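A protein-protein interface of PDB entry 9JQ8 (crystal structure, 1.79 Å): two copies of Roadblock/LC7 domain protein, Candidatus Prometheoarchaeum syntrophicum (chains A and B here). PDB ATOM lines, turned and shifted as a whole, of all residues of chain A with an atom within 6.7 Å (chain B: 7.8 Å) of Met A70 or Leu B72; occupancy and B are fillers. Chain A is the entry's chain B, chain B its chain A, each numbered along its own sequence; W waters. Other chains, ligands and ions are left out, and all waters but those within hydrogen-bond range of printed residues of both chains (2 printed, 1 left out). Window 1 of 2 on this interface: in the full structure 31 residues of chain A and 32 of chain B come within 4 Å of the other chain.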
ATOM      1  N   SER A  50       7.240  18.145  20.254  1.00  0.00           N
ATOM      2  CA  SER A  50       7.573  18.915  19.052  1.00  0.00           C
ATOM      3  C   SER A  50       7.234  18.145  17.784  1.00  0.00           C
ATOM      4  O   SER A  50       6.698  18.714  16.824  1.00  0.00           O
ATOM      5  CB  SER A  50       9.057  19.277  19.042  1.00  0.00           C
ATOM      6  OG  SER A  50       9.407  20.144  20.100  1.00  0.00           O
ATOM      7  N   VAL A  51       7.557  16.852  17.755  1.00  0.00           N
ATOM      8  CA  VAL A  51       7.285  16.049  16.571  1.00  0.00           C
ATOM      9  C   VAL A  51       5.786  15.840  16.389  1.00  0.00           C
ATOM     10  O   VAL A  51       5.282  15.836  15.256  1.00  0.00           O
ATOM     11  CB  VAL A  51       8.075  14.734  16.670  1.00  0.00           C
ATOM     12  CG1 VAL A  51       7.659  13.733  15.614  1.00  0.00           C
ATOM     13  CG2 VAL A  51       9.572  15.051  16.595  1.00  0.00           C
ATOM     14  N   SER A  52       5.050  15.673  17.492  1.00  0.00           N
ATOM     15  CA  SER A  52       3.591  15.646  17.435  1.00  0.00           C
ATOM     16  C   SER A  52       3.040  16.870  16.725  1.00  0.00           C
ATOM     17  O   SER A  52       2.141  16.759  15.886  1.00  0.00           O
ATOM     18  CB  SER A  52       2.996  15.561  18.838  1.00  0.00           C
ATOM     19  OG  SER A  52       1.579  15.669  18.782  1.00  0.00           O
ATOM     20  N   MET A  54       4.599  18.951  14.611  1.00  0.00           N
ATOM     21  CA  MET A  54       4.965  18.918  13.198  1.00  0.00           C
ATOM     22  C   MET A  54       4.057  17.990  12.403  1.00  0.00           C
ATOM     23  O   MET A  54       3.666  18.312  11.272  1.00  0.00           O
ATOM     24  CB  MET A  54       6.416  18.483  13.045  1.00  0.00           C
ATOM     25  CG  MET A  54       7.412  19.484  13.546  1.00  0.00           C
ATOM     26  SD  MET A  54       9.100  18.939  13.231  1.00  0.00           S
ATOM     27  CE  MET A  54       9.203  19.193  11.471  1.00  0.00           C
ATOM     28  N   PHE A  55       3.734  16.819  12.960  1.00  0.00           N
ATOM     29  CA  PHE A  55       2.832  15.908  12.266  1.00  0.00           C
ATOM     30  C   PHE A  55       1.454  16.515  12.059  1.00  0.00           C
ATOM     31  O   PHE A  55       0.694  16.021  11.225  1.00  0.00           O
ATOM     32  CB  PHE A  55       2.672  14.597  13.032  1.00  0.00           C
ATOM     33  CG  PHE A  55       3.637  13.520  12.613  1.00  0.00           C
ATOM     34  CD1 PHE A  55       3.701  13.104  11.288  1.00  0.00           C
ATOM     35  CD2 PHE A  55       4.458  12.915  13.540  1.00  0.00           C
ATOM     36  CE1 PHE A  55       4.582  12.100  10.897  1.00  0.00           C
ATOM     37  CE2 PHE A  55       5.330  11.912  13.166  1.00  0.00           C
ATOM     38  CZ  PHE A  55       5.398  11.494  11.858  1.00  0.00           C
ATOM     39  N   THR A  57       0.926  19.590  11.078  1.00  0.00           N
ATOM     40  CA  THR A  57       1.009  20.640  10.066  1.00  0.00           C
ATOM     41  C   THR A  57       0.039  20.377   8.927  1.00  0.00           C
ATOM     42  O   THR A  57       0.048  19.301   8.323  1.00  0.00           O
ATOM     43  CB  THR A  57       2.432  20.742   9.518  1.00  0.00           C
ATOM     44  OG1 THR A  57       3.325  21.110  10.576  1.00  0.00           O
ATOM     45  CG2 THR A  57       2.495  21.790   8.412  1.00  0.00           C
ATOM     46  N   ILE A  59      -0.701  21.271   5.294  1.00  0.00           N
ATOM     47  CA  ILE A  59      -0.257  21.883   4.053  1.00  0.00           C
ATOM     48  C   ILE A  59      -1.391  21.701   3.053  1.00  0.00           C
ATOM     49  O   ILE A  59      -1.253  20.992   2.050  1.00  0.00           O
ATOM     50  CB  ILE A  59       1.078  21.280   3.582  1.00  0.00           C
ATOM     51  CG1 ILE A  59       1.054  19.759   3.677  1.00  0.00           C
ATOM     52  CG2 ILE A  59       2.213  21.770   4.468  1.00  0.00           C
ATOM     53  CD1 ILE A  59       2.457  19.152   3.679  1.00  0.00           C
ATOM     54  N   LEU A  67       0.170  14.031   6.856  1.00  0.00           N
ATOM     55  CA  LEU A  67       1.573  13.671   6.997  1.00  0.00           C
ATOM     56  C   LEU A  67       1.676  12.352   7.750  1.00  0.00           C
ATOM     57  O   LEU A  67       1.062  12.191   8.808  1.00  0.00           O
ATOM     58  CB  LEU A  67       2.302  14.786   7.742  1.00  0.00           C
ATOM     59  CG  LEU A  67       3.814  14.906   7.835  1.00  0.00           C
ATOM     60  CD1 LEU A  67       4.485  14.668   6.505  1.00  0.00           C
ATOM     61  CD2 LEU A  67       4.167  16.298   8.377  1.00  0.00           C
ATOM     62  N   LEU A  68       2.435  11.409   7.202  1.00  0.00           N
ATOM     63  CA  LEU A  68       2.582  10.090   7.806  1.00  0.00           C
ATOM     64  C   LEU A  68       4.021   9.733   8.157  1.00  0.00           C
ATOM     65  O   LEU A  68       4.243   8.917   9.056  1.00  0.00           O
ATOM     66  CB  LEU A  68       2.010   9.003   6.873  1.00  0.00           C
ATOM     67  CG  LEU A  68       0.594   9.218   6.344  1.00  0.00           C
ATOM     68  CD1 LEU A  68       0.295   8.181   5.293  1.00  0.00           C
ATOM     69  CD2 LEU A  68      -0.390   9.095   7.489  1.00  0.00           C
ATOM     70  N   GLU A  69       5.005  10.327   7.495  1.00  0.00           N
ATOM     71  CA  GLU A  69       6.388  10.075   7.858  1.00  0.00           C
ATOM     72  C   GLU A  69       7.200  11.331   7.615  1.00  0.00           C
ATOM     73  O   GLU A  69       6.893  12.130   6.727  1.00  0.00           O
ATOM     74  CB  GLU A  69       6.986   8.896   7.083  1.00  0.00           C
ATOM     75  CG  GLU A  69       6.884   9.005   5.583  1.00  0.00           C
ATOM     76  CD  GLU A  69       7.192   7.695   4.892  1.00  0.00           C
ATOM     77  OE1 GLU A  69       7.009   6.628   5.524  1.00  0.00           O
ATOM     78  OE2 GLU A  69       7.622   7.730   3.722  1.00  0.00           O
ATOM     79  N   MET A  70       8.239  11.509   8.420  1.00  0.00           N
ATOM     80  CA  MET A  70       9.094  12.671   8.287  1.00  0.00           C
ATOM     81  C   MET A  70      10.533  12.229   8.452  1.00  0.00           C
ATOM     82  O   MET A  70      10.853  11.451   9.356  1.00  0.00           O
ATOM     83  CB  MET A  70       8.763  13.750   9.326  1.00  0.00           C
ATOM     84  CG  MET A  70       7.366  14.349   9.220  1.00  0.00           C
ATOM     85  SD  MET A  70       7.244  15.749  10.354  1.00  0.00           S
ATOM     86  CE  MET A  70       7.865  14.964  11.829  1.00  0.00           C
ATOM     87  N   THR A  71      11.395  12.730   7.576  1.00  0.00           N
ATOM     88  CA  THR A  71      12.834  12.609   7.741  1.00  0.00           C
ATOM     89  C   THR A  71      13.394  14.019   7.845  1.00  0.00           C
ATOM     90  O   THR A  71      13.247  14.815   6.914  1.00  0.00           O
ATOM     91  CB  THR A  71      13.470  11.856   6.577  1.00  0.00           C
ATOM     92  OG1 THR A  71      12.905  10.550   6.493  1.00  0.00           O
ATOM     93  CG2 THR A  71      14.954  11.745   6.763  1.00  0.00           C
ATOM     94  N   LEU A  72      13.995  14.340   8.986  1.00  0.00           N
ATOM     95  CA  LEU A  72      14.486  15.687   9.254  1.00  0.00           C
ATOM     96  C   LEU A  72      16.008  15.648   9.270  1.00  0.00           C
ATOM     97  O   LEU A  72      16.596  14.902  10.061  1.00  0.00           O
ATOM     98  CB  LEU A  72      13.947  16.205  10.588  1.00  0.00           C
ATOM     99  CG  LEU A  72      12.426  16.153  10.757  1.00  0.00           C
ATOM    100  CD1 LEU A  72      12.037  16.684  12.127  1.00  0.00           C
ATOM    101  CD2 LEU A  72      11.702  16.922   9.656  1.00  0.00           C
ATOM    102  N   LEU A  79      16.428  13.033  12.382  1.00  0.00           N
ATOM    103  CA  LEU A  79      15.302  12.434  13.083  1.00  0.00           C
ATOM    104  C   LEU A  79      14.400  11.830  12.027  1.00  0.00           C
ATOM    105  O   LEU A  79      14.091  12.484  11.030  1.00  0.00           O
ATOM    106  CB  LEU A  79      14.551  13.470  13.925  1.00  0.00           C
ATOM    107  CG  LEU A  79      13.340  13.020  14.752  1.00  0.00           C
ATOM    108  CD1 LEU A  79      13.140  13.987  15.881  1.00  0.00           C
ATOM    109  CD2 LEU A  79      12.090  12.995  13.901  1.00  0.00           C
ATOM    110  N   ILE A  80      14.008  10.581  12.230  1.00  0.00           N
ATOM    111  CA  ILE A  80      13.028   9.915  11.384  1.00  0.00           C
ATOM    112  C   ILE A  80      11.805   9.657  12.249  1.00  0.00           C
ATOM    113  O   ILE A  80      11.936   9.224  13.401  1.00  0.00           O
ATOM    114  CB  ILE A  80      13.598   8.609  10.816  1.00  0.00           C
ATOM    115  CG1 ILE A  80      14.765   8.905   9.880  1.00  0.00           C
ATOM    116  CG2 ILE A  80      12.494   7.788  10.128  1.00  0.00           C
ATOM    117  CD1 ILE A  80      15.655   7.712   9.646  1.00  0.00           C
ATOM    118  N   ALA A  81      10.627   9.982  11.735  1.00  0.00           N
ATOM    119  CA  ALA A  81       9.391   9.790  12.478  1.00  0.00           C
ATOM    120  C   ALA A  81       8.383   9.122  11.563  1.00  0.00           C
ATOM    121  O   ALA A  81       8.223   9.540  10.410  1.00  0.00           O
ATOM    122  CB  ALA A  81       8.840  11.123  12.995  1.00  0.00           C
ATOM    123  N   VAL A  82       7.726   8.071  12.061  1.00  0.00           N
ATOM    124  CA  VAL A  82       6.690   7.360  11.319  1.00  0.00           C
ATOM    125  C   VAL A  82       5.483   7.245  12.236  1.00  0.00           C
ATOM    126  O   VAL A  82       5.633   6.863  13.396  1.00  0.00           O
ATOM    127  CB  VAL A  82       7.138   5.946  10.891  1.00  0.00           C
ATOM    128  CG1 VAL A  82       6.035   5.263  10.083  1.00  0.00           C
ATOM    129  CG2 VAL A  82       8.439   5.984  10.104  1.00  0.00           C
ATOM    130  N   LYS A  83       4.292   7.525  11.722  1.00  0.00           N
ATOM    131  CA  LYS A  83       3.103   7.435  12.550  1.00  0.00           C
ATOM    132  C   LYS A  83       2.069   6.547  11.874  1.00  0.00           C
ATOM    133  O   LYS A  83       2.041   6.410  10.648  1.00  0.00           O
ATOM    134  CB  LYS A  83       2.493   8.828  12.834  1.00  0.00           C
ATOM    135  CG  LYS A  83       1.846   9.491  11.609  1.00  0.00           C
ATOM    136  CD  LYS A  83       1.186  10.830  11.936  1.00  0.00           C
ATOM    137  CE  LYS A  83      -0.279  10.674  12.319  1.00  0.00           C
ATOM    138  NZ  LYS A  83      -0.805  11.940  12.941  1.00  0.00           N
ATOM    139  N   LEU A 105      14.217   4.234   8.328  1.00  0.00           N
ATOM    140  CA  LEU A 105      12.849   4.579   7.960  1.00  0.00           C
ATOM    141  C   LEU A 105      12.077   3.342   7.537  1.00  0.00           C
ATOM    142  O   LEU A 105      10.908   3.168   7.903  1.00  0.00           O
ATOM    143  CB  LEU A 105      12.862   5.616   6.832  1.00  0.00           C
ATOM    144  CG  LEU A 105      11.497   5.873   6.209  1.00  0.00           C
ATOM    145  CD1 LEU A 105      10.584   6.497   7.249  1.00  0.00           C
ATOM    146  CD2 LEU A 105      11.644   6.789   5.011  1.00  0.00           C
ATOM    147  N   SER B  50       3.412  27.469   4.532  1.00  0.00           N
ATOM    148  CA  SER B  50       3.286  26.322   5.428  1.00  0.00           C
ATOM    149  C   SER B  50       4.647  25.706   5.729  1.00  0.00           C
ATOM    150  O   SER B  50       4.988  25.455   6.893  1.00  0.00           O
ATOM    151  CB  SER B  50       2.355  25.278   4.810  1.00  0.00           C
ATOM    152  OG  SER B  50       1.025  25.758   4.737  1.00  0.00           O
ATOM    153  N   VAL B  51       5.436  25.454   4.682  1.00  0.00           N
ATOM    154  CA  VAL B  51       6.747  24.837   4.849  1.00  0.00           C
ATOM    155  C   VAL B  51       7.694  25.765   5.603  1.00  0.00           C
ATOM    156  O   VAL B  51       8.446  25.324   6.483  1.00  0.00           O
ATOM    157  CB  VAL B  51       7.314  24.441   3.478  1.00  0.00           C
ATOM    158  CG1 VAL B  51       8.737  23.918   3.623  1.00  0.00           C
ATOM    159  CG2 VAL B  51       6.411  23.407   2.825  1.00  0.00           C
ATOM    160  N   MET B  54       7.042  25.373   9.118  1.00  0.00           N
ATOM    161  CA  MET B  54       7.576  24.088   9.564  1.00  0.00           C
ATOM    162  C   MET B  54       9.071  24.162   9.814  1.00  0.00           C
ATOM    163  O   MET B  54       9.577  23.561  10.772  1.00  0.00           O
ATOM    164  CB  MET B  54       7.313  23.000   8.531  1.00  0.00           C
ATOM    165  CG  MET B  54       5.982  22.325   8.624  1.00  0.00           C
ATOM    166  SD  MET B  54       6.043  20.825   7.644  1.00  0.00           S
ATOM    167  CE  MET B  54       6.726  19.642   8.812  1.00  0.00           C
ATOM    168  N   GLU B  69      16.800  20.193   6.224  1.00  0.00           N
ATOM    169  CA  GLU B  69      16.147  19.449   5.153  1.00  0.00           C
ATOM    170  C   GLU B  69      14.961  18.700   5.730  1.00  0.00           C
ATOM    171  O   GLU B  69      15.018  18.207   6.853  1.00  0.00           O
ATOM    172  CB  GLU B  69      17.058  18.393   4.509  1.00  0.00           C
ATOM    173  CG  GLU B  69      18.410  18.867   4.098  1.00  0.00           C
ATOM    174  CD  GLU B  69      19.431  17.739   4.051  1.00  0.00           C
ATOM    175  OE1 GLU B  69      20.617  18.050   3.809  1.00  0.00           O
ATOM    176  OE2 GLU B  69      19.064  16.556   4.267  1.00  0.00           O
ATOM    177  N   MET B  70      13.901  18.578   4.942  1.00  0.00           N
ATOM    178  CA  MET B  70      12.761  17.772   5.348  1.00  0.00           C
ATOM    179  C   MET B  70      12.324  16.918   4.168  1.00  0.00           C
ATOM    180  O   MET B  70      12.264  17.407   3.039  1.00  0.00           O
ATOM    181  CB  MET B  70      11.600  18.650   5.812  1.00  0.00           C
ATOM    182  CG  MET B  70      11.887  19.492   7.037  1.00  0.00           C
ATOM    183  SD  MET B  70      10.425  20.429   7.551  1.00  0.00           S
ATOM    184  CE  MET B  70       9.927  21.165   5.992  1.00  0.00           C
ATOM    185  N   THR B  71      12.032  15.647   4.430  1.00  0.00           N
ATOM    186  CA  THR B  71      11.405  14.752   3.466  1.00  0.00           C
ATOM    187  C   THR B  71      10.097  14.313   4.106  1.00  0.00           C
ATOM    188  O   THR B  71      10.116  13.648   5.152  1.00  0.00           O
ATOM    189  CB  THR B  71      12.289  13.541   3.162  1.00  0.00           C
ATOM    190  OG1 THR B  71      13.561  13.975   2.668  1.00  0.00           O
ATOM    191  CG2 THR B  71      11.614  12.637   2.115  1.00  0.00           C
ATOM    192  N   LEU B  72       8.976  14.732   3.527  1.00  0.00           N
ATOM    193  CA  LEU B  72       7.660  14.518   4.110  1.00  0.00           C
ATOM    194  C   LEU B  72       6.899  13.483   3.302  1.00  0.00           C
ATOM    195  O   LEU B  72       6.669  13.675   2.106  1.00  0.00           O
ATOM    196  CB  LEU B  72       6.870  15.824   4.160  1.00  0.00           C
ATOM    197  CG  LEU B  72       7.544  16.951   4.944  1.00  0.00           C
ATOM    198  CD1 LEU B  72       6.637  18.185   5.015  1.00  0.00           C
ATOM    199  CD2 LEU B  72       7.929  16.473   6.337  1.00  0.00           C
ATOM    200  N   GLY B  73       6.518  12.380   3.950  1.00  0.00           N
ATOM    201  CA  GLY B  73       5.695  11.375   3.318  1.00  0.00           C
ATOM    202  C   GLY B  73       4.240  11.619   3.643  1.00  0.00           C
ATOM    203  O   GLY B  73       3.851  11.667   4.813  1.00  0.00           O
ATOM    204  N   MET B  74       3.431  11.791   2.605  1.00  0.00           N
ATOM    205  CA  MET B  74       2.029  12.147   2.748  1.00  0.00           C
ATOM    206  C   MET B  74       1.153  11.006   2.264  1.00  0.00           C
ATOM    207  O   MET B  74       1.628  10.024   1.695  1.00  0.00           O
ATOM    208  CB  MET B  74       1.697  13.412   1.947  1.00  0.00           C
ATOM    209  CG  MET B  74       2.815  14.404   1.871  1.00  0.00           C
ATOM    210  SD  MET B  74       2.737  15.408   3.334  1.00  0.00           S
ATOM    211  CE  MET B  74       1.070  16.035   3.140  1.00  0.00           C
ATOM    212  N   ASP B  75      -0.150  11.167   2.486  1.00  0.00           N
ATOM    213  CA  ASP B  75      -1.116  10.204   1.971  1.00  0.00           C
ATOM    214  C   ASP B  75      -0.979  10.046   0.466  1.00  0.00           C
ATOM    215  O   ASP B  75      -1.091   8.938  -0.069  1.00  0.00           O
ATOM    216  CB  ASP B  75      -2.530  10.664   2.298  1.00  0.00           C
ATOM    217  CG  ASP B  75      -3.012  10.203   3.657  1.00  0.00           C
ATOM    218  OD1 ASP B  75      -2.818   9.018   3.990  1.00  0.00           O
ATOM    219  OD2 ASP B  75      -3.644  11.025   4.367  1.00  0.00           O
ATOM    220  N   GLY B  77       1.659  11.257  -1.631  1.00  0.00           N
ATOM    221  CA  GLY B  77       2.962  11.527  -2.210  1.00  0.00           C
ATOM    222  C   GLY B  77       3.999  12.061  -1.242  1.00  0.00           C
ATOM    223  O   GLY B  77       4.039  11.636  -0.085  1.00  0.00           O
ATOM    224  N   PHE B  78       4.847  12.979  -1.704  1.00  0.00           N
ATOM    225  CA  PHE B  78       6.008  13.417  -0.945  1.00  0.00           C
ATOM    226  C   PHE B  78       6.242  14.903  -1.141  1.00  0.00           C
ATOM    227  O   PHE B  78       6.002  15.446  -2.221  1.00  0.00           O
ATOM    228  CB  PHE B  78       7.271  12.673  -1.370  1.00  0.00           C
ATOM    229  CG  PHE B  78       7.143  11.191  -1.257  1.00  0.00           C
ATOM    230  CD1 PHE B  78       6.599  10.454  -2.299  1.00  0.00           C
ATOM    231  CD2 PHE B  78       7.552  10.533  -0.111  1.00  0.00           C
ATOM    232  CE1 PHE B  78       6.466   9.084  -2.199  1.00  0.00           C
ATOM    233  CE2 PHE B  78       7.412   9.162  -0.005  1.00  0.00           C
ATOM    234  CZ  PHE B  78       6.876   8.443  -1.055  1.00  0.00           C
ATOM    235  N   LEU B  79       6.740  15.551  -0.094  1.00  0.00           N
ATOM    236  CA  LEU B  79       7.281  16.898  -0.209  1.00  0.00           C
ATOM    237  C   LEU B  79       8.701  16.895   0.335  1.00  0.00           C
ATOM    238  O   LEU B  79       8.931  16.482   1.478  1.00  0.00           O
ATOM    239  CB  LEU B  79       6.414  17.918   0.541  1.00  0.00           C
ATOM    240  CG  LEU B  79       6.796  19.392   0.334  1.00  0.00           C
ATOM    241  CD1 LEU B  79       5.581  20.265   0.587  1.00  0.00           C
ATOM    242  CD2 LEU B  79       7.919  19.827   1.276  1.00  0.00           C
ATOM    243  N   ILE B  80       9.638  17.383  -0.472  1.00  0.00           N
ATOM    244  CA  ILE B  80      11.035  17.490  -0.089  1.00  0.00           C
ATOM    245  C   ILE B  80      11.377  18.972  -0.024  1.00  0.00           C
ATOM    246  O   ILE B  80      11.014  19.734  -0.932  1.00  0.00           O
ATOM    247  CB  ILE B  80      11.944  16.762  -1.089  1.00  0.00           C
ATOM    248  CG1 ILE B  80      11.619  15.276  -1.130  1.00  0.00           C
ATOM    249  CG2 ILE B  80      13.412  17.032  -0.768  1.00  0.00           C
ATOM    250  CD1 ILE B  80      12.432  14.514  -2.161  1.00  0.00           C
ATOM    251  N   ALA B  81      12.054  19.389   1.042  1.00  0.00           N
ATOM    252  CA  ALA B  81      12.406  20.794   1.208  1.00  0.00           C
ATOM    253  C   ALA B  81      13.820  20.910   1.750  1.00  0.00           C
ATOM    254  O   ALA B  81      14.223  20.164   2.645  1.00  0.00           O
ATOM    255  CB  ALA B  81      11.438  21.523   2.153  1.00  0.00           C
ATOM    256  N   GLY B  91      10.162  20.458  -3.487  1.00  0.00           N
ATOM    257  CA  GLY B  91       9.774  19.613  -4.601  1.00  0.00           C
ATOM    258  C   GLY B  91       8.657  18.681  -4.185  1.00  0.00           C
ATOM    259  O   GLY B  91       8.570  18.276  -3.034  1.00  0.00           O
ATOM    260  N   LEU B  93       6.337  15.143  -5.190  1.00  0.00           N
ATOM    261  CA  LEU B  93       6.250  13.880  -5.909  1.00  0.00           C
ATOM    262  C   LEU B  93       4.913  13.226  -5.611  1.00  0.00           C
ATOM    263  O   LEU B  93       4.356  13.402  -4.530  1.00  0.00           O
ATOM    264  CB  LEU B  93       7.365  12.907  -5.517  1.00  0.00           C
ATOM    265  CG  LEU B  93       8.788  13.293  -5.871  1.00  0.00           C
ATOM    266  CD1 LEU B  93       9.773  12.489  -5.071  1.00  0.00           C
ATOM    267  CD2 LEU B  93       8.995  13.055  -7.353  1.00  0.00           C
ATOM    268  N   ARG B  98       8.296   7.335  -4.947  1.00  0.00           N
ATOM    269  CA  ARG B  98       9.234   7.078  -3.858  1.00  0.00           C
ATOM    270  C   ARG B  98      10.596   6.639  -4.388  1.00  0.00           C
ATOM    271  O   ARG B  98      11.626   6.897  -3.753  1.00  0.00           O
ATOM    272  CB  ARG B  98       8.677   6.020  -2.883  1.00  0.00           C
ATOM    273  CG  ARG B  98       9.452   6.023  -1.546  1.00  0.00           C
ATOM    274  CD  ARG B  98       9.157   4.866  -0.564  1.00  0.00           C
ATOM    275  NE  ARG B  98       7.947   5.124   0.219  1.00  0.00           N
ATOM    276  CZ  ARG B  98       7.937   5.698   1.419  1.00  0.00           C
ATOM    277  NH1 ARG B  98       9.061   6.047   2.029  1.00  0.00           N
ATOM    278  NH2 ARG B  98       6.774   5.918   2.025  1.00  0.00           N
ATOM    279  N   VAL B 101      12.723   9.754  -4.599  1.00  0.00           N
ATOM    280  CA  VAL B 101      12.861  10.666  -3.464  1.00  0.00           C
ATOM    281  C   VAL B 101      14.328  11.005  -3.221  1.00  0.00           C
ATOM    282  O   VAL B 101      14.693  12.172  -3.035  1.00  0.00           O
ATOM    283  CB  VAL B 101      12.206  10.078  -2.200  1.00  0.00           C
ATOM    284  CG1 VAL B 101      12.635  10.866  -0.985  1.00  0.00           C
ATOM    285  CG2 VAL B 101      10.698  10.122  -2.314  1.00  0.00           C
HETATM  286  O   HOH W   1      15.169  15.007   4.704  1.00  0.00           O
HETATM  287  O   HOH W   2      10.221  10.711   5.280  1.00  0.00           O
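Of the printed residues of chain B, Met A54 touches Met B54.
Met A70 touches just these residues of chain B: Thr B71 and Leu B72.
Printed residues of chain A within 4 Å of Leu B72: Leu A67 (3.5 Å), Glu A69 (3.6 Å) and Met A70 (3.6 Å).
Of the printed residues of chain A, Gly B73 touches Leu A67, Leu A68 and Glu A69.
Of the printed residues of chain A, Phe B78 touches Glu A69 (3.998 Å).
Leu B79 touches none of the printed residues of chain A.
The nearest residue of chain B that does not touch Met A70 is Met B54 (4.2 Å).
The nearest residue of chain A that does not touch Leu B72 is Ile A59 (4.5 Å).
The nearest printed residue of chain A that does not touch Ser B50 is Thr A57 (4.7 Å).
Among the printed residues, merely in contact across the chains: Thr A71 with Met B70 (3.4 Å), Met A70 with Thr B71 (3.4 Å), Ile A59 with Met B74 (3.5 Å), Leu A68 with Asp B75 (3.5 Å), Leu A67 with Gly B73 (3.5 Å), Thr A57 with Met B54 (3.5 Å), Leu A72 with Glu B69 (3.5 Å), Ile A59 with Ser B50 (3.5 Å), Leu A67 with Leu B72 (3.5 Å), Glu A69 with Leu B72 (3.6 Å), Met A70 with Leu B72 (3.6 Å), Met A54 with Met B54 (3.7 Å), Leu A72 with Met B70 (3.7 Å), Leu A67 with Met B74 (3.7 Å), Thr A71 with Glu B69 (3.8 Å), Glu A69 with Thr B71 (3.9 Å) and Glu A69 with Phe B78 (3.998 Å).
The backbone NH (N) of Thr B71 is in hydrogen-bond range of the backbone carbonyl oxygen (O) of Thr A71 (2.9 Å).
O of Gly B73 is in hydrogen-bond range of N of Leu A68, at 2.8 Å.
The backbone carbonyl oxygen (O) of Glu A69 sits at hydrogen-bond distance from the backbone NH (N) of Gly B73, 2.8 Å away.
NH2 of Arg B98 is in salt-bridge range of OE2 of Glu A69.
Water W1 bridges OG1 of Thr B71 and O of Thr A71.
Water W2 bridges O of Thr B71 and OG1 of Thr A71.
Of the 19 printed residues of chain A, 9 touch a printed residue of chain B.
Hydrophobic or aromatic side chains of chain A that line the printed part of chain B: Met A54, Ile A59, Leu A67, Leu A68, Met A70 and Leu A72.
Among the printed residues, 21 pairs touch across the chains.
Met A54 touches its own counterpart, Met B54.
Glu A69 touches Thr B71, and with the chains exchanged Thr A71 touches Glu B69.
Met A70 touches Thr B71, and with the chains exchanged Thr A71 touches Met B70.
Met A70 touches Leu B72, and with the chains exchanged Leu A72 touches Met B70.
10 positions are printed for both chains.
The backbone NH of Met B70 is in hydrogen-bond range of the backbone carbonyl oxygen of Ala B81 (2.8 Å).
O of Leu B79 sits at hydrogen-bond distance from N of Leu B72 (2.7 Å).
The side-chain hydroxyl of Thr A57 is in hydrogen-bond range of the backbone carbonyl oxygen of Met A54 (2.9 Å).
O of Leu A68 sits at hydrogen-bond distance from N of Lys A83, 3.0 Å away.
The backbone carbonyl oxygen (O) of Ala A81 sits at hydrogen-bond distance from the backbone NH (N) of Met A70 (2.8 Å).
O of Leu A79 sits at hydrogen-bond distance from N of Leu A72, 2.8 Å away.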
